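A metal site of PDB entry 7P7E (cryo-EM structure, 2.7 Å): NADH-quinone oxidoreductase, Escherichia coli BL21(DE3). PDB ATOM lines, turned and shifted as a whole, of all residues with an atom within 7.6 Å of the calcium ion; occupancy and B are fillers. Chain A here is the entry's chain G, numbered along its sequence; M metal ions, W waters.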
ATOM      1  N   GLU A 614      34.679  -3.818  -5.309  1.00  0.00           N
ATOM      2  CA  GLU A 614      33.682  -4.803  -4.947  1.00  0.00           C
ATOM      3  C   GLU A 614      33.454  -4.886  -3.441  1.00  0.00           C
ATOM      4  O   GLU A 614      32.872  -5.855  -2.961  1.00  0.00           O
ATOM      5  CB  GLU A 614      34.075  -6.174  -5.493  1.00  0.00           C
ATOM      6  CG  GLU A 614      34.456  -6.163  -6.952  1.00  0.00           C
ATOM      7  CD  GLU A 614      35.905  -6.579  -7.182  1.00  0.00           C
ATOM      8  OE1 GLU A 614      36.680  -6.553  -6.211  1.00  0.00           O
ATOM      9  OE2 GLU A 614      36.245  -6.928  -8.327  1.00  0.00           O
ATOM     10  N   SER A 615      33.881  -3.864  -2.690  1.00  0.00           N
ATOM     11  CA  SER A 615      33.746  -3.890  -1.242  1.00  0.00           C
ATOM     12  C   SER A 615      33.382  -2.499  -0.731  1.00  0.00           C
ATOM     13  O   SER A 615      33.586  -1.488  -1.412  1.00  0.00           O
ATOM     14  CB  SER A 615      35.036  -4.364  -0.572  1.00  0.00           C
ATOM     15  OG  SER A 615      36.122  -3.496  -0.856  1.00  0.00           O
ATOM     16  N   ASP A 616      32.828  -2.475   0.474  1.00  0.00           N
ATOM     17  CA  ASP A 616      32.617  -1.252   1.226  1.00  0.00           C
ATOM     18  C   ASP A 616      33.620  -1.202   2.374  1.00  0.00           C
ATOM     19  O   ASP A 616      34.194  -2.218   2.768  1.00  0.00           O
ATOM     20  CB  ASP A 616      31.193  -1.186   1.790  1.00  0.00           C
ATOM     21  CG  ASP A 616      30.152  -1.607   0.765  1.00  0.00           C
ATOM     22  OD1 ASP A 616      29.869  -0.820  -0.155  1.00  0.00           O
ATOM     23  OD2 ASP A 616      29.618  -2.722   0.897  1.00  0.00           O
ATOM     24  N   PHE A 630      32.391   2.886  -1.105  1.00  0.00           N
ATOM     25  CA  PHE A 630      31.224   2.058  -1.356  1.00  0.00           C
ATOM     26  C   PHE A 630      31.504   1.093  -2.501  1.00  0.00           C
ATOM     27  O   PHE A 630      32.330   1.382  -3.384  1.00  0.00           O
ATOM     28  CB  PHE A 630      29.990   2.920  -1.681  1.00  0.00           C
ATOM     29  CG  PHE A 630      29.621   3.888  -0.591  1.00  0.00           C
ATOM     30  CD1 PHE A 630      30.220   5.130  -0.499  1.00  0.00           C
ATOM     31  CD2 PHE A 630      28.650   3.563   0.338  1.00  0.00           C
ATOM     32  CE1 PHE A 630      29.868   6.022   0.495  1.00  0.00           C
ATOM     33  CE2 PHE A 630      28.297   4.440   1.346  1.00  0.00           C
ATOM     34  CZ  PHE A 630      28.902   5.677   1.417  1.00  0.00           C
ATOM     35  N   GLN A 631      30.826  -0.048  -2.476  1.00  0.00           N
ATOM     36  CA  GLN A 631      30.977  -1.047  -3.526  1.00  0.00           C
ATOM     37  C   GLN A 631      30.403  -0.525  -4.838  1.00  0.00           C
ATOM     38  O   GLN A 631      29.338   0.093  -4.870  1.00  0.00           O
ATOM     39  CB  GLN A 631      30.278  -2.340  -3.104  1.00  0.00           C
ATOM     40  CG  GLN A 631      30.285  -3.439  -4.149  1.00  0.00           C
ATOM     41  CD  GLN A 631      29.803  -4.759  -3.594  1.00  0.00           C
ATOM     42  OE1 GLN A 631      29.597  -4.899  -2.386  1.00  0.00           O
ATOM     43  NE2 GLN A 631      29.614  -5.739  -4.460  1.00  0.00           N
ATOM     44  N   VAL A 632      31.134  -0.776  -5.925  1.00  0.00           N
ATOM     45  CA  VAL A 632      30.696  -0.305  -7.245  1.00  0.00           C
ATOM     46  C   VAL A 632      29.765  -1.301  -7.903  1.00  0.00           C
ATOM     47  O   VAL A 632      28.709  -0.925  -8.424  1.00  0.00           O
ATOM     48  CB  VAL A 632      31.922  -0.016  -8.133  1.00  0.00           C
ATOM     49  CG1 VAL A 632      31.507   0.778  -9.362  1.00  0.00           C
ATOM     50  CG2 VAL A 632      32.976   0.739  -7.350  1.00  0.00           C
ATOM     51  N   TYR A 633      30.122  -2.579  -7.902  1.00  0.00           N
ATOM     52  CA  TYR A 633      29.329  -3.583  -8.594  1.00  0.00           C
ATOM     53  C   TYR A 633      29.379  -4.888  -7.813  1.00  0.00           C
ATOM     54  O   TYR A 633      30.293  -5.118  -7.015  1.00  0.00           O
ATOM     55  CB  TYR A 633      29.818  -3.792 -10.028  1.00  0.00           C
ATOM     56  CG  TYR A 633      31.165  -4.461 -10.146  1.00  0.00           C
ATOM     57  CD1 TYR A 633      32.345  -3.736  -9.963  1.00  0.00           C
ATOM     58  CD2 TYR A 633      31.276  -5.812 -10.455  1.00  0.00           C
ATOM     59  CE1 TYR A 633      33.577  -4.343 -10.074  1.00  0.00           C
ATOM     60  CE2 TYR A 633      32.506  -6.427 -10.559  1.00  0.00           C
ATOM     61  CZ  TYR A 633      33.653  -5.686 -10.377  1.00  0.00           C
ATOM     62  OH  TYR A 633      34.874  -6.301 -10.485  1.00  0.00           O
ATOM     63  N   ASP A 634      28.396  -5.733  -8.073  1.00  0.00           N
ATOM     64  CA  ASP A 634      28.385  -7.086  -7.532  1.00  0.00           C
ATOM     65  C   ASP A 634      29.191  -7.985  -8.458  1.00  0.00           C
ATOM     66  O   ASP A 634      28.828  -8.127  -9.635  1.00  0.00           O
ATOM     67  CB  ASP A 634      26.970  -7.606  -7.403  1.00  0.00           C
ATOM     68  CG  ASP A 634      26.824  -8.657  -6.325  1.00  0.00           C
ATOM     69  OD1 ASP A 634      27.575  -9.656  -6.366  1.00  0.00           O
ATOM     70  OD2 ASP A 634      25.966  -8.493  -5.440  1.00  0.00           O
ATOM     71  N   GLU A 646      33.520  -9.356   0.967  1.00  0.00           N
ATOM     72  CA  GLU A 646      34.309  -8.381   1.686  1.00  0.00           C
ATOM     73  C   GLU A 646      35.204  -9.067   2.697  1.00  0.00           C
ATOM     74  O   GLU A 646      34.890 -10.148   3.211  1.00  0.00           O
ATOM     75  CB  GLU A 646      33.405  -7.378   2.398  1.00  0.00           C
ATOM     76  CG  GLU A 646      32.836  -6.311   1.494  1.00  0.00           C
ATOM     77  CD  GLU A 646      31.443  -6.647   0.992  1.00  0.00           C
ATOM     78  OE1 GLU A 646      31.076  -7.843   0.983  1.00  0.00           O
ATOM     79  OE2 GLU A 646      30.719  -5.710   0.610  1.00  0.00           O
ATOM     80  N   TRP A 648      36.077  -8.021   5.763  1.00  0.00           N
ATOM     81  CA  TRP A 648      35.436  -8.061   7.080  1.00  0.00           C
ATOM     82  C   TRP A 648      34.270  -9.037   7.115  1.00  0.00           C
ATOM     83  O   TRP A 648      34.018  -9.631   8.159  1.00  0.00           O
ATOM     84  CB  TRP A 648      34.991  -6.659   7.503  1.00  0.00           C
ATOM     85  CG  TRP A 648      34.423  -5.804   6.410  1.00  0.00           C
ATOM     86  CD1 TRP A 648      35.091  -4.917   5.640  1.00  0.00           C
ATOM     87  CD2 TRP A 648      33.050  -5.731   6.002  1.00  0.00           C
ATOM     88  NE1 TRP A 648      34.241  -4.305   4.763  1.00  0.00           N
ATOM     89  CE2 TRP A 648      32.978  -4.790   4.967  1.00  0.00           C
ATOM     90  CE3 TRP A 648      31.879  -6.377   6.400  1.00  0.00           C
ATOM     91  CZ2 TRP A 648      31.775  -4.476   4.327  1.00  0.00           C
ATOM     92  CZ3 TRP A 648      30.695  -6.060   5.766  1.00  0.00           C
ATOM     93  CH2 TRP A 648      30.655  -5.122   4.731  1.00  0.00           C
ATOM     94  N   ARG A 649      33.598  -9.246   5.986  1.00  0.00           N
ATOM     95  CA  ARG A 649      32.554 -10.267   5.913  1.00  0.00           C
ATOM     96  C   ARG A 649      33.151 -11.662   6.086  1.00  0.00           C
ATOM     97  O   ARG A 649      32.628 -12.478   6.864  1.00  0.00           O
ATOM     98  CB  ARG A 649      31.796 -10.157   4.600  1.00  0.00           C
ATOM     99  CG  ARG A 649      30.539 -10.994   4.521  1.00  0.00           C
ATOM    100  CD  ARG A 649      29.585 -10.473   3.470  1.00  0.00           C
ATOM    101  NE  ARG A 649      28.515  -9.693   4.063  1.00  0.00           N
ATOM    102  CZ  ARG A 649      28.174  -8.472   3.673  1.00  0.00           C
ATOM    103  NH1 ARG A 649      28.787  -7.862   2.681  1.00  0.00           N
ATOM    104  NH2 ARG A 649      27.178  -7.845   4.301  1.00  0.00           N
ATOM    105  N   LEU A 668      27.402  -4.264   7.368  1.00  0.00           N
ATOM    106  CA  LEU A 668      28.534  -3.338   7.512  1.00  0.00           C
ATOM    107  C   LEU A 668      28.381  -2.428   8.718  1.00  0.00           C
ATOM    108  O   LEU A 668      29.356  -2.162   9.429  1.00  0.00           O
ATOM    109  CB  LEU A 668      28.687  -2.504   6.225  1.00  0.00           C
ATOM    110  CG  LEU A 668      29.606  -1.273   6.303  1.00  0.00           C
ATOM    111  CD1 LEU A 668      31.055  -1.674   6.464  1.00  0.00           C
ATOM    112  CD2 LEU A 668      29.425  -0.374   5.087  1.00  0.00           C
ATOM    113  N   ARG A 703      23.129   4.142  -8.225  1.00  0.00           N
ATOM    114  CA  ARG A 703      24.508   3.925  -8.633  1.00  0.00           C
ATOM    115  C   ARG A 703      24.735   4.129 -10.125  1.00  0.00           C
ATOM    116  O   ARG A 703      25.881   4.315 -10.541  1.00  0.00           O
ATOM    117  CB  ARG A 703      24.948   2.504  -8.271  1.00  0.00           C
ATOM    118  CG  ARG A 703      25.589   2.362  -6.904  1.00  0.00           C
ATOM    119  CD  ARG A 703      26.198   0.990  -6.749  1.00  0.00           C
ATOM    120  NE  ARG A 703      26.814   0.781  -5.445  1.00  0.00           N
ATOM    121  CZ  ARG A 703      26.214   0.208  -4.410  1.00  0.00           C
ATOM    122  NH1 ARG A 703      24.963  -0.214  -4.494  1.00  0.00           N
ATOM    123  NH2 ARG A 703      26.884   0.053  -3.279  1.00  0.00           N
ATOM    124  N   GLN A 727      21.044  -6.990  -4.309  1.00  0.00           N
ATOM    125  CA  GLN A 727      20.610  -6.233  -3.146  1.00  0.00           C
ATOM    126  C   GLN A 727      21.814  -5.757  -2.352  1.00  0.00           C
ATOM    127  O   GLN A 727      22.789  -6.498  -2.168  1.00  0.00           O
ATOM    128  CB  GLN A 727      19.707  -7.097  -2.265  1.00  0.00           C
ATOM    129  CG  GLN A 727      18.524  -7.700  -3.002  1.00  0.00           C
ATOM    130  CD  GLN A 727      17.619  -6.650  -3.613  1.00  0.00           C
ATOM    131  OE1 GLN A 727      17.101  -5.777  -2.902  1.00  0.00           O
ATOM    132  NE2 GLN A 727      17.433  -6.708  -4.927  1.00  0.00           N
ATOM    133  N   ASP A 728      21.753  -4.507  -1.910  1.00  0.00           N
ATOM    134  CA  ASP A 728      22.801  -3.889  -1.115  1.00  0.00           C
ATOM    135  C   ASP A 728      22.254  -3.638   0.282  1.00  0.00           C
ATOM    136  O   ASP A 728      21.636  -2.602   0.533  1.00  0.00           O
ATOM    137  CB  ASP A 728      23.294  -2.601  -1.765  1.00  0.00           C
ATOM    138  CG  ASP A 728      24.622  -2.139  -1.208  1.00  0.00           C
ATOM    139  OD1 ASP A 728      25.394  -2.978  -0.712  1.00  0.00           O
ATOM    140  OD2 ASP A 728      24.898  -0.920  -1.261  1.00  0.00           O
ATOM    141  N   ILE A 729      22.470  -4.592   1.189  1.00  0.00           N
ATOM    142  CA  ILE A 729      22.116  -4.385   2.594  1.00  0.00           C
ATOM    143  C   ILE A 729      23.200  -3.653   3.354  1.00  0.00           C
ATOM    144  O   ILE A 729      22.956  -3.190   4.473  1.00  0.00           O
ATOM    145  CB  ILE A 729      21.817  -5.724   3.289  1.00  0.00           C
ATOM    146  CG1 ILE A 729      23.023  -6.670   3.174  1.00  0.00           C
ATOM    147  CG2 ILE A 729      20.573  -6.366   2.709  1.00  0.00           C
ATOM    148  CD1 ILE A 729      23.433  -7.294   4.484  1.00  0.00           C
ATOM    149  N   ASP A 730      24.402  -3.536   2.781  1.00  0.00           N
ATOM    150  CA  ASP A 730      25.515  -2.908   3.492  1.00  0.00           C
ATOM    151  C   ASP A 730      25.381  -1.399   3.552  1.00  0.00           C
ATOM    152  O   ASP A 730      25.632  -0.792   4.599  1.00  0.00           O
ATOM    153  CB  ASP A 730      26.828  -3.294   2.813  1.00  0.00           C
ATOM    154  CG  ASP A 730      27.235  -4.726   3.114  1.00  0.00           C
ATOM    155  OD1 ASP A 730      27.009  -5.183   4.254  1.00  0.00           O
ATOM    156  OD2 ASP A 730      27.780  -5.385   2.209  1.00  0.00           O
ATOM    157  N   THR A 731      24.992  -0.753   2.448  1.00  0.00           N
ATOM    158  CA  THR A 731      25.023   0.697   2.330  1.00  0.00           C
ATOM    159  C   THR A 731      23.665   1.222   1.871  1.00  0.00           C
ATOM    160  O   THR A 731      22.730   0.462   1.623  1.00  0.00           O
ATOM    161  CB  THR A 731      26.111   1.174   1.362  1.00  0.00           C
ATOM    162  OG1 THR A 731      25.725   0.881   0.015  1.00  0.00           O
ATOM    163  CG2 THR A 731      27.453   0.513   1.655  1.00  0.00           C
ATOM    164  N   PHE A 735      21.905  -1.027  -6.377  1.00  0.00           N
ATOM    165  CA  PHE A 735      22.618  -1.464  -7.568  1.00  0.00           C
ATOM    166  C   PHE A 735      21.746  -1.357  -8.811  1.00  0.00           C
ATOM    167  O   PHE A 735      21.597  -2.304  -9.575  1.00  0.00           O
ATOM    168  CB  PHE A 735      23.109  -2.897  -7.376  1.00  0.00           C
ATOM    169  CG  PHE A 735      24.328  -3.019  -6.522  1.00  0.00           C
ATOM    170  CD1 PHE A 735      25.564  -2.620  -6.988  1.00  0.00           C
ATOM    171  CD2 PHE A 735      24.241  -3.558  -5.244  1.00  0.00           C
ATOM    172  CE1 PHE A 735      26.695  -2.726  -6.202  1.00  0.00           C
ATOM    173  CE2 PHE A 735      25.374  -3.677  -4.458  1.00  0.00           C
ATOM    174  CZ  PHE A 735      26.599  -3.258  -4.934  1.00  0.00           C
HETATM  175 CA    CA M   1      28.554  -4.747  -0.105  1.00  0.00          CA
HETATM  176  O   HOH W   1      27.565  -6.920  -1.006  1.00  0.00           O
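The calcium ion is bound by the side-chain carboxylate (OE2) of Glu 646 (2.5 Å), the side-chain carboxylate (OD2) of Asp 616 (2.5 Å), the side-chain amide oxygen (OE1) of Gln 631 (2.5 Å), the side-chain carboxylate (OD2) of Asp 730 (2.5 Å) and water W1 (2.6 Å).
Asp 728 touches the calcium ion. The nearest printed residue that does not touch the calcium ion is Arg 649 (4.2 Å).
O of Asp 616 lies within hydrogen-bond range of NE1 of Trp 648, 2.9 Å away. The backbone NH of Leu 668 is in hydrogen-bond range of the side-chain carboxylate of Asp 730, 3.3 Å away. NH2 of Arg 703 is in salt-bridge range of OD2 of Asp 728 (3.0 Å). The side-chain carboxylate (OD1) of Asp 730 lies within salt-bridge range of the guanidinium group (NH2) of Arg 649. The backbone carbonyl oxygen (O) of Gln 631 sits at hydrogen-bond distance from the guanidinium group (NE) of Arg 703, at 2.7 Å. The backbone NH of Gln 631 lies within hydrogen-bond range of the backbone carbonyl oxygen of Ser 615, at 3.3 Å. The backbone carbonyl oxygen (O) of Glu 614 lies close to the side-chain amide oxygen (OE1) of Gln 631, at 3.5 Å. NE2 of Gln 631 sits at hydrogen-bond distance from O of Tyr 633.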
